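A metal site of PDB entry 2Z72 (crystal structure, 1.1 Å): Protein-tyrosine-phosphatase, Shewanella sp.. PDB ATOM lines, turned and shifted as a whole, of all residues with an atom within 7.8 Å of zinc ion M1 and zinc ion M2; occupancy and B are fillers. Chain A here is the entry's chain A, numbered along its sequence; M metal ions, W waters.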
ATOM      1  N   SER A  77     -22.271  15.636  -4.872  1.00  0.00           N
ATOM      2  CA  SER A  77     -23.200  16.539  -5.550  1.00  0.00           C
ATOM      3  C   SER A  77     -22.526  17.300  -6.663  1.00  0.00           C
ATOM      4  O   SER A  77     -21.311  17.377  -6.762  1.00  0.00           O
ATOM      5  CB  SER A  77     -23.655  17.572  -4.527  1.00  0.00           C
ATOM      6  OG  SER A  77     -24.846  18.222  -4.928  1.00  0.00           O
ATOM      7  N   ASP A  78     -23.338  17.893  -7.513  1.00  0.00           N
ATOM      8  CA  ASP A  78     -22.917  18.907  -8.486  1.00  0.00           C
ATOM      9  C   ASP A  78     -21.828  18.389  -9.418  1.00  0.00           C
ATOM     10  O   ASP A  78     -20.822  19.021  -9.708  1.00  0.00           O
ATOM     11  CB  ASP A  78     -22.468  20.188  -7.765  1.00  0.00           C
ATOM     12  CG  ASP A  78     -23.630  20.883  -7.073  1.00  0.00           C
ATOM     13  OD1 ASP A  78     -24.301  21.757  -7.650  1.00  0.00           O
ATOM     14  OD2 ASP A  78     -23.925  20.466  -5.907  1.00  0.00           O
ATOM     15  N   VAL A  79     -22.086  17.180  -9.969  1.00  0.00           N
ATOM     16  CA  VAL A  79     -21.152  16.629 -10.946  1.00  0.00           C
ATOM     17  C   VAL A  79     -21.098  17.485 -12.225  1.00  0.00           C
ATOM     18  O   VAL A  79     -20.047  17.549 -12.839  1.00  0.00           O
ATOM     19  CB  VAL A  79     -21.552  15.159 -11.213  1.00  0.00           C
ATOM     20  CG1 VAL A  79     -20.814  14.568 -12.389  1.00  0.00           C
ATOM     21  CG2 VAL A  79     -21.355  14.305  -9.968  1.00  0.00           C
ATOM     22  N   HIS A  80     -22.225  18.077 -12.625  1.00  0.00           N
ATOM     23  CA  HIS A  80     -22.216  19.033 -13.743  1.00  0.00           C
ATOM     24  C   HIS A  80     -21.511  18.470 -14.958  1.00  0.00           C
ATOM     25  O   HIS A  80     -20.580  19.032 -15.529  1.00  0.00           O
ATOM     26  CB  HIS A  80     -21.620  20.387 -13.292  1.00  0.00           C
ATOM     27  CG  HIS A  80     -22.617  21.163 -12.490  1.00  0.00           C
ATOM     28  ND1 HIS A  80     -23.839  21.519 -12.982  1.00  0.00           N
ATOM     29  CD2 HIS A  80     -22.562  21.701 -11.243  1.00  0.00           C
ATOM     30  CE1 HIS A  80     -24.501  22.193 -12.065  1.00  0.00           C
ATOM     31  NE2 HIS A  80     -23.760  22.346 -10.955  1.00  0.00           N
ATOM     32  N   THR A 112     -26.925  14.792  -4.302  1.00  0.00           N
ATOM     33  CA  THR A 112     -27.842  15.900  -4.037  1.00  0.00           C
ATOM     34  C   THR A 112     -27.989  16.867  -5.193  1.00  0.00           C
ATOM     35  O   THR A 112     -27.959  18.098  -4.980  1.00  0.00           O
ATOM     36  CB  THR A 112     -27.466  16.641  -2.747  1.00  0.00           C
ATOM     37  OG1 THR A 112     -26.148  17.115  -2.822  1.00  0.00           O
ATOM     38  CG2 THR A 112     -27.501  15.694  -1.519  1.00  0.00           C
ATOM     39  N   GLY A 113     -28.182  16.350  -6.418  1.00  0.00           N
ATOM     40  CA  GLY A 113     -28.536  17.193  -7.556  1.00  0.00           C
ATOM     41  C   GLY A 113     -27.383  17.655  -8.433  1.00  0.00           C
ATOM     42  O   GLY A 113     -26.212  17.453  -8.178  1.00  0.00           O
ATOM     43  N   ASP A 114     -27.803  18.264  -9.536  1.00  0.00           N
ATOM     44  CA  ASP A 114     -26.917  18.973 -10.492  1.00  0.00           C
ATOM     45  C   ASP A 114     -25.947  18.082 -11.204  1.00  0.00           C
ATOM     46  O   ASP A 114     -24.755  18.328 -11.337  1.00  0.00           O
ATOM     47  CB  ASP A 114     -26.233  20.170  -9.835  1.00  0.00           C
ATOM     48  CG  ASP A 114     -27.080  21.413  -9.791  1.00  0.00           C
ATOM     49  OD1 ASP A 114     -26.448  22.517  -9.444  1.00  0.00           O
ATOM     50  OD2 ASP A 114     -28.294  21.359 -10.039  1.00  0.00           O
ATOM     51  N   ILE A 115     -26.524  17.006 -11.806  1.00  0.00           N
ATOM     52  CA  ILE A 115     -25.863  16.265 -12.872  1.00  0.00           C
ATOM     53  C   ILE A 115     -25.741  17.109 -14.131  1.00  0.00           C
ATOM     54  O   ILE A 115     -24.715  17.151 -14.799  1.00  0.00           O
ATOM     55  CB  ILE A 115     -26.607  14.960 -13.193  1.00  0.00           C
ATOM     56  CG1 ILE A 115     -26.436  13.959 -12.056  1.00  0.00           C
ATOM     57  CG2 ILE A 115     -26.138  14.403 -14.537  1.00  0.00           C
ATOM     58  CD1 ILE A 115     -27.257  12.694 -12.182  1.00  0.00           C
ATOM     59  N   PHE A 116     -26.842  17.770 -14.501  1.00  0.00           N
ATOM     60  CA  PHE A 116     -26.872  18.562 -15.733  1.00  0.00           C
ATOM     61  C   PHE A 116     -26.000  19.819 -15.665  1.00  0.00           C
ATOM     62  O   PHE A 116     -25.742  20.368 -14.606  1.00  0.00           O
ATOM     63  CB  PHE A 116     -28.274  19.006 -16.035  1.00  0.00           C
ATOM     64  CG  PHE A 116     -29.198  17.925 -16.538  1.00  0.00           C
ATOM     65  CD1 PHE A 116     -30.028  17.211 -15.682  1.00  0.00           C
ATOM     66  CD2 PHE A 116     -29.227  17.635 -17.884  1.00  0.00           C
ATOM     67  CE1 PHE A 116     -30.853  16.246 -16.186  1.00  0.00           C
ATOM     68  CE2 PHE A 116     -30.053  16.669 -18.358  1.00  0.00           C
ATOM     69  CZ  PHE A 116     -30.884  15.988 -17.539  1.00  0.00           C
ATOM     70  N   ASP A 117     -25.617  20.235 -16.867  1.00  0.00           N
ATOM     71  CA  ASP A 117     -25.110  21.547 -17.251  1.00  0.00           C
ATOM     72  C   ASP A 117     -23.626  21.723 -16.937  1.00  0.00           C
ATOM     73  O   ASP A 117     -23.029  21.024 -16.132  1.00  0.00           O
ATOM     74  CB  ASP A 117     -25.970  22.649 -16.627  1.00  0.00           C
ATOM     75  CG  ASP A 117     -27.355  22.756 -17.234  1.00  0.00           C
ATOM     76  OD1 ASP A 117     -28.185  23.516 -16.646  1.00  0.00           O
ATOM     77  OD2 ASP A 117     -27.601  22.135 -18.291  1.00  0.00           O
ATOM     78  N   GLY A 148     -31.704  18.751  -8.403  1.00  0.00           N
ATOM     79  CA  GLY A 148     -31.118  20.045  -8.146  1.00  0.00           C
ATOM     80  C   GLY A 148     -31.711  21.115  -8.974  1.00  0.00           C
ATOM     81  O   GLY A 148     -32.638  20.903  -9.793  1.00  0.00           O
ATOM     82  N   ASN A 149     -31.202  22.360  -8.847  1.00  0.00           N
ATOM     83  CA  ASN A 149     -31.756  23.426  -9.652  1.00  0.00           C
ATOM     84  C   ASN A 149     -31.503  23.209 -11.138  1.00  0.00           C
ATOM     85  O   ASN A 149     -32.390  23.587 -11.922  1.00  0.00           O
ATOM     86  CB  ASN A 149     -31.268  24.827  -9.196  1.00  0.00           C
ATOM     87  CG  ASN A 149     -29.816  25.067  -9.319  1.00  0.00           C
ATOM     88  OD1 ASN A 149     -29.001  24.254  -8.877  1.00  0.00           O
ATOM     89  ND2 ASN A 149     -29.388  26.206  -9.822  1.00  0.00           N
ATOM     90  N   HIS A 150     -30.377  22.607 -11.507  1.00  0.00           N
ATOM     91  CA  HIS A 150     -30.186  22.393 -12.961  1.00  0.00           C
ATOM     92  C   HIS A 150     -31.058  21.304 -13.523  1.00  0.00           C
ATOM     93  O   HIS A 150     -31.470  21.404 -14.696  1.00  0.00           O
ATOM     94  CB  HIS A 150     -28.723  22.170 -13.274  1.00  0.00           C
ATOM     95  CG  HIS A 150     -27.961  23.473 -13.139  1.00  0.00           C
ATOM     96  ND1 HIS A 150     -27.631  24.230 -14.248  1.00  0.00           N
ATOM     97  CD2 HIS A 150     -27.539  24.114 -12.042  1.00  0.00           C
ATOM     98  CE1 HIS A 150     -27.021  25.290 -13.798  1.00  0.00           C
ATOM     99  NE2 HIS A 150     -26.921  25.292 -12.476  1.00  0.00           N
ATOM    100  N   GLU A 151     -31.420  20.253 -12.792  1.00  0.00           N
ATOM    101  CA  GLU A 151     -32.441  19.324 -13.270  1.00  0.00           C
ATOM    102  C   GLU A 151     -33.745  20.052 -13.546  1.00  0.00           C
ATOM    103  O   GLU A 151     -34.411  19.825 -14.548  1.00  0.00           O
ATOM    104  CB  GLU A 151     -32.664  18.162 -12.310  1.00  0.00           C
ATOM    105  CG  GLU A 151     -31.590  17.110 -12.269  1.00  0.00           C
ATOM    106  CD  GLU A 151     -30.260  17.611 -11.771  1.00  0.00           C
ATOM    107  OE1 GLU A 151     -29.222  17.312 -12.375  1.00  0.00           O
ATOM    108  OE2 GLU A 151     -30.292  18.296 -10.720  1.00  0.00           O
ATOM    109  N   MET A 153     -34.229  23.284 -14.088  1.00  0.00           N
ATOM    110  CA  MET A 153     -34.062  24.228 -15.198  1.00  0.00           C
ATOM    111  C   MET A 153     -34.149  23.497 -16.541  1.00  0.00           C
ATOM    112  O   MET A 153     -34.929  23.849 -17.410  1.00  0.00           O
ATOM    113  CB  MET A 153     -32.740  24.972 -15.089  1.00  0.00           C
ATOM    114  CG  MET A 153     -32.957  26.213 -14.199  1.00  0.00           C
ATOM    115  SD  MET A 153     -31.578  27.353 -14.240  1.00  0.00           S
ATOM    116  CE  MET A 153     -30.332  26.517 -13.287  1.00  0.00           C
ATOM    117  N   HIS A 207     -30.494  19.916  -2.295  1.00  0.00           N
ATOM    118  CA  HIS A 207     -29.489  20.561  -3.116  1.00  0.00           C
ATOM    119  C   HIS A 207     -28.967  21.878  -2.557  1.00  0.00           C
ATOM    120  O   HIS A 207     -27.748  22.069  -2.455  1.00  0.00           O
ATOM    121  CB  HIS A 207     -30.064  20.748  -4.520  1.00  0.00           C
ATOM    122  CG  HIS A 207     -29.057  21.338  -5.456  1.00  0.00           C
ATOM    123  ND1 HIS A 207     -27.929  20.625  -5.810  1.00  0.00           N
ATOM    124  CD2 HIS A 207     -28.972  22.520  -6.074  1.00  0.00           C
ATOM    125  CE1 HIS A 207     -27.195  21.370  -6.586  1.00  0.00           C
ATOM    126  NE2 HIS A 207     -27.788  22.561  -6.808  1.00  0.00           N
ATOM    127  N   GLY A 208     -29.846  22.803  -2.224  1.00  0.00           N
ATOM    128  CA  GLY A 208     -29.493  24.160  -1.820  1.00  0.00           C
ATOM    129  C   GLY A 208     -29.475  24.355  -0.333  1.00  0.00           C
ATOM    130  O   GLY A 208     -28.451  24.648   0.296  1.00  0.00           O
ATOM    131  N   THR A 255     -33.935  24.163  -3.629  1.00  0.00           N
ATOM    132  CA  THR A 255     -32.947  23.885  -4.661  1.00  0.00           C
ATOM    133  C   THR A 255     -32.102  25.074  -5.083  1.00  0.00           C
ATOM    134  O   THR A 255     -31.131  24.887  -5.807  1.00  0.00           O
ATOM    135  CB  THR A 255     -33.594  23.266  -5.903  1.00  0.00           C
ATOM    136  OG1 THR A 255     -34.572  24.178  -6.383  1.00  0.00           O
ATOM    137  CG2 THR A 255     -34.221  21.928  -5.573  1.00  0.00           C
ATOM    138  N   TRP A 256     -32.365  26.259  -4.537  1.00  0.00           N
ATOM    139  CA  TRP A 256     -31.553  27.443  -4.842  1.00  0.00           C
ATOM    140  C   TRP A 256     -30.981  28.114  -3.627  1.00  0.00           C
ATOM    141  O   TRP A 256     -30.037  28.906  -3.751  1.00  0.00           O
ATOM    142  CB  TRP A 256     -32.381  28.475  -5.604  1.00  0.00           C
ATOM    143  CG  TRP A 256     -32.668  28.169  -7.027  1.00  0.00           C
ATOM    144  CD1 TRP A 256     -33.711  27.430  -7.534  1.00  0.00           C
ATOM    145  CD2 TRP A 256     -31.907  28.570  -8.149  1.00  0.00           C
ATOM    146  NE1 TRP A 256     -33.660  27.369  -8.891  1.00  0.00           N
ATOM    147  CE2 TRP A 256     -32.546  28.056  -9.307  1.00  0.00           C
ATOM    148  CE3 TRP A 256     -30.764  29.327  -8.342  1.00  0.00           C
ATOM    149  CZ2 TRP A 256     -32.068  28.285 -10.604  1.00  0.00           C
ATOM    150  CZ3 TRP A 256     -30.294  29.540  -9.601  1.00  0.00           C
ATOM    151  CH2 TRP A 256     -30.926  29.018 -10.736  1.00  0.00           C
ATOM    152  N   ARG A 258     -29.012  29.652  -0.745  1.00  0.00           N
ATOM    153  CA  ARG A 258     -27.615  29.673  -0.411  1.00  0.00           C
ATOM    154  C   ARG A 258     -27.317  30.297   0.951  1.00  0.00           C
ATOM    155  O   ARG A 258     -26.184  30.634   1.261  1.00  0.00           O
ATOM    156  CB  ARG A 258     -26.726  30.417  -1.445  1.00  0.00           C
ATOM    157  CG  ARG A 258     -26.769  29.696  -2.761  1.00  0.00           C
ATOM    158  CD  ARG A 258     -25.662  30.235  -3.619  1.00  0.00           C
ATOM    159  NE  ARG A 258     -25.812  29.918  -4.988  1.00  0.00           N
ATOM    160  CZ  ARG A 258     -25.359  29.051  -5.803  1.00  0.00           C
ATOM    161  NH1 ARG A 258     -25.549  28.849  -7.124  1.00  0.00           N
ATOM    162  NH2 ARG A 258     -24.531  28.143  -5.276  1.00  0.00           N
ATOM    163  N   GLY A 285     -25.525  20.612  -1.454  1.00  0.00           N
ATOM    164  CA  GLY A 285     -24.625  20.882  -2.584  1.00  0.00           C
ATOM    165  C   GLY A 285     -24.728  22.338  -2.986  1.00  0.00           C
ATOM    166  O   GLY A 285     -24.722  23.232  -2.079  1.00  0.00           O
ATOM    167  N   HIS A 286     -24.832  22.613  -4.284  1.00  0.00           N
ATOM    168  CA  HIS A 286     -25.204  23.825  -4.952  1.00  0.00           C
ATOM    169  C   HIS A 286     -24.202  24.957  -4.905  1.00  0.00           C
ATOM    170  O   HIS A 286     -24.012  25.634  -5.925  1.00  0.00           O
ATOM    171  CB  HIS A 286     -26.581  24.325  -4.459  1.00  0.00           C
ATOM    172  CG  HIS A 286     -27.172  25.496  -5.152  1.00  0.00           C
ATOM    173  ND1 HIS A 286     -27.477  25.605  -6.481  1.00  0.00           N
ATOM    174  CD2 HIS A 286     -27.588  26.684  -4.613  1.00  0.00           C
ATOM    175  CE1 HIS A 286     -27.996  26.787  -6.670  1.00  0.00           C
ATOM    176  NE2 HIS A 286     -28.102  27.503  -5.563  1.00  0.00           N
ATOM    177  N   THR A 287     -23.647  25.241  -3.760  1.00  0.00           N
ATOM    178  CA  THR A 287     -22.686  26.285  -3.507  1.00  0.00           C
ATOM    179  C   THR A 287     -21.289  25.660  -3.407  1.00  0.00           C
ATOM    180  O   THR A 287     -20.974  24.999  -2.422  1.00  0.00           O
ATOM    181  CB  THR A 287     -23.068  27.097  -2.252  1.00  0.00           C
ATOM    182  OG1 THR A 287     -24.417  27.534  -2.356  1.00  0.00           O
ATOM    183  CG2 THR A 287     -22.152  28.343  -2.161  1.00  0.00           C
ATOM    184  N   SER A 288     -20.484  25.882  -4.480  1.00  0.00           N
ATOM    185  CA  SER A 288     -19.295  25.077  -4.670  1.00  0.00           C
ATOM    186  C   SER A 288     -18.193  25.464  -3.680  1.00  0.00           C
ATOM    187  O   SER A 288     -17.875  26.636  -3.521  1.00  0.00           O
ATOM    188  CB  SER A 288     -18.773  25.216  -6.084  1.00  0.00           C
ATOM    189  OG  SER A 288     -19.833  24.983  -7.014  1.00  0.00           O
ATOM    190  N   ASP A 304     -20.818  20.010  -2.384  1.00  0.00           N
ATOM    191  CA  ASP A 304     -20.388  20.438  -3.717  1.00  0.00           C
ATOM    192  C   ASP A 304     -18.897  20.718  -3.575  1.00  0.00           C
ATOM    193  O   ASP A 304     -18.544  21.762  -3.000  1.00  0.00           O
ATOM    194  CB  ASP A 304     -21.182  21.597  -4.223  1.00  0.00           C
ATOM    195  CG  ASP A 304     -20.730  22.092  -5.602  1.00  0.00           C
ATOM    196  OD1 ASP A 304     -21.450  22.942  -6.146  1.00  0.00           O
ATOM    197  OD2 ASP A 304     -19.674  21.590  -6.094  1.00  0.00           O
ATOM    198  N   LYS A 308     -17.453  20.268 -10.846  1.00  0.00           N
ATOM    199  CA  LYS A 308     -17.783  20.967 -12.075  1.00  0.00           C
ATOM    200  C   LYS A 308     -16.565  21.527 -12.765  1.00  0.00           C
ATOM    201  O   LYS A 308     -16.618  21.738 -13.962  1.00  0.00           O
ATOM    202  CB  LYS A 308     -18.780  22.102 -11.821  1.00  0.00           C
ATOM    203  CG  LYS A 308     -18.177  23.291 -11.043  1.00  0.00           C
ATOM    204  CD  LYS A 308     -19.172  24.293 -10.608  1.00  0.00           C
ATOM    205  CE  LYS A 308     -18.520  25.473  -9.911  1.00  0.00           C
ATOM    206  NZ  LYS A 308     -19.483  26.491  -9.484  1.00  0.00           N
HETATM  207 ZN    ZN M   1     -27.162  24.091  -7.948  1.00  0.00          ZN
HETATM  208 ZN    ZN M   2     -24.357  23.038  -9.172  1.00  0.00          ZN
HETATM  209  O   HOH W   1     -25.341  24.592  -8.472  1.00  0.00           O
HETATM  210  O   HOH W   2     -22.435  23.755  -8.636  1.00  0.00           O
HETATM  211  O   HOH W   3     -26.466  26.639 -10.080  1.00  0.00           O
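Zinc ion M2 is bound by water W1 (2.0 Å), the side-chain carboxylate (OD1) of Asp 78 (2.0 Å), a ring nitrogen (NE2) of His 80 (2.0 Å), water W2 (2.1 Å) and the side-chain carboxylate (OD1) of Asp 114 (2.2 Å).
Zinc ion M1 is bound by water W1 (2.0 Å), NE2 of His 207 (2.0 Å), OD1 of Asn 149 (2.1 Å), ND1 of His 286 (2.1 Å) and OD1 of Asp 114 (2.3 Å).
Zinc ion M1 has five donor atoms within binding distance.
Of the 26 residues printed, 3 come within 4 Å of zinc ion M2.
The nearest printed residue that does not touch zinc ion M2 is His 286 (4.2 Å).
Water W2 lies within hydrogen-bond range of OD1 of Asp 304 (2.8 Å) and OG of Ser 288 (3.3 Å).
Water W3 lies within hydrogen-bond range of a ring nitrogen (NE2) of His 150 and the side-chain amide nitrogen of Asn 149.
The nearest printed residue that does not touch zinc ion M1 is His 150 (4.1 Å).
N of Asp 78 sits at hydrogen-bond distance from O of Gly 113, 3.0 Å away.
The side-chain hydroxyl of Ser 77 sits at hydrogen-bond distance from the side-chain carboxylate of Asp 78, at 2.6 Å.
The backbone NH (N) of His 80 lies close to the backbone carbonyl oxygen (O) of Ile 115, at 3.4 Å.
ND1 of His 80 sits close to O of Asp 117, 3.3 Å away.
The backbone NH of Gly 285 lies within hydrogen-bond range of the backbone carbonyl oxygen of His 207 (2.8 Å).
The backbone carbonyl oxygen (O) of His 286 is in hydrogen-bond range of the guanidinium group (NH2) of Arg 258 (2.6 Å).
N of Val 79 lies within hydrogen-bond range of O of Asp 114, 3.2 Å away.
The backbone NH of Asp 114 is in hydrogen-bond range of the side-chain carboxylate of Glu 151.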
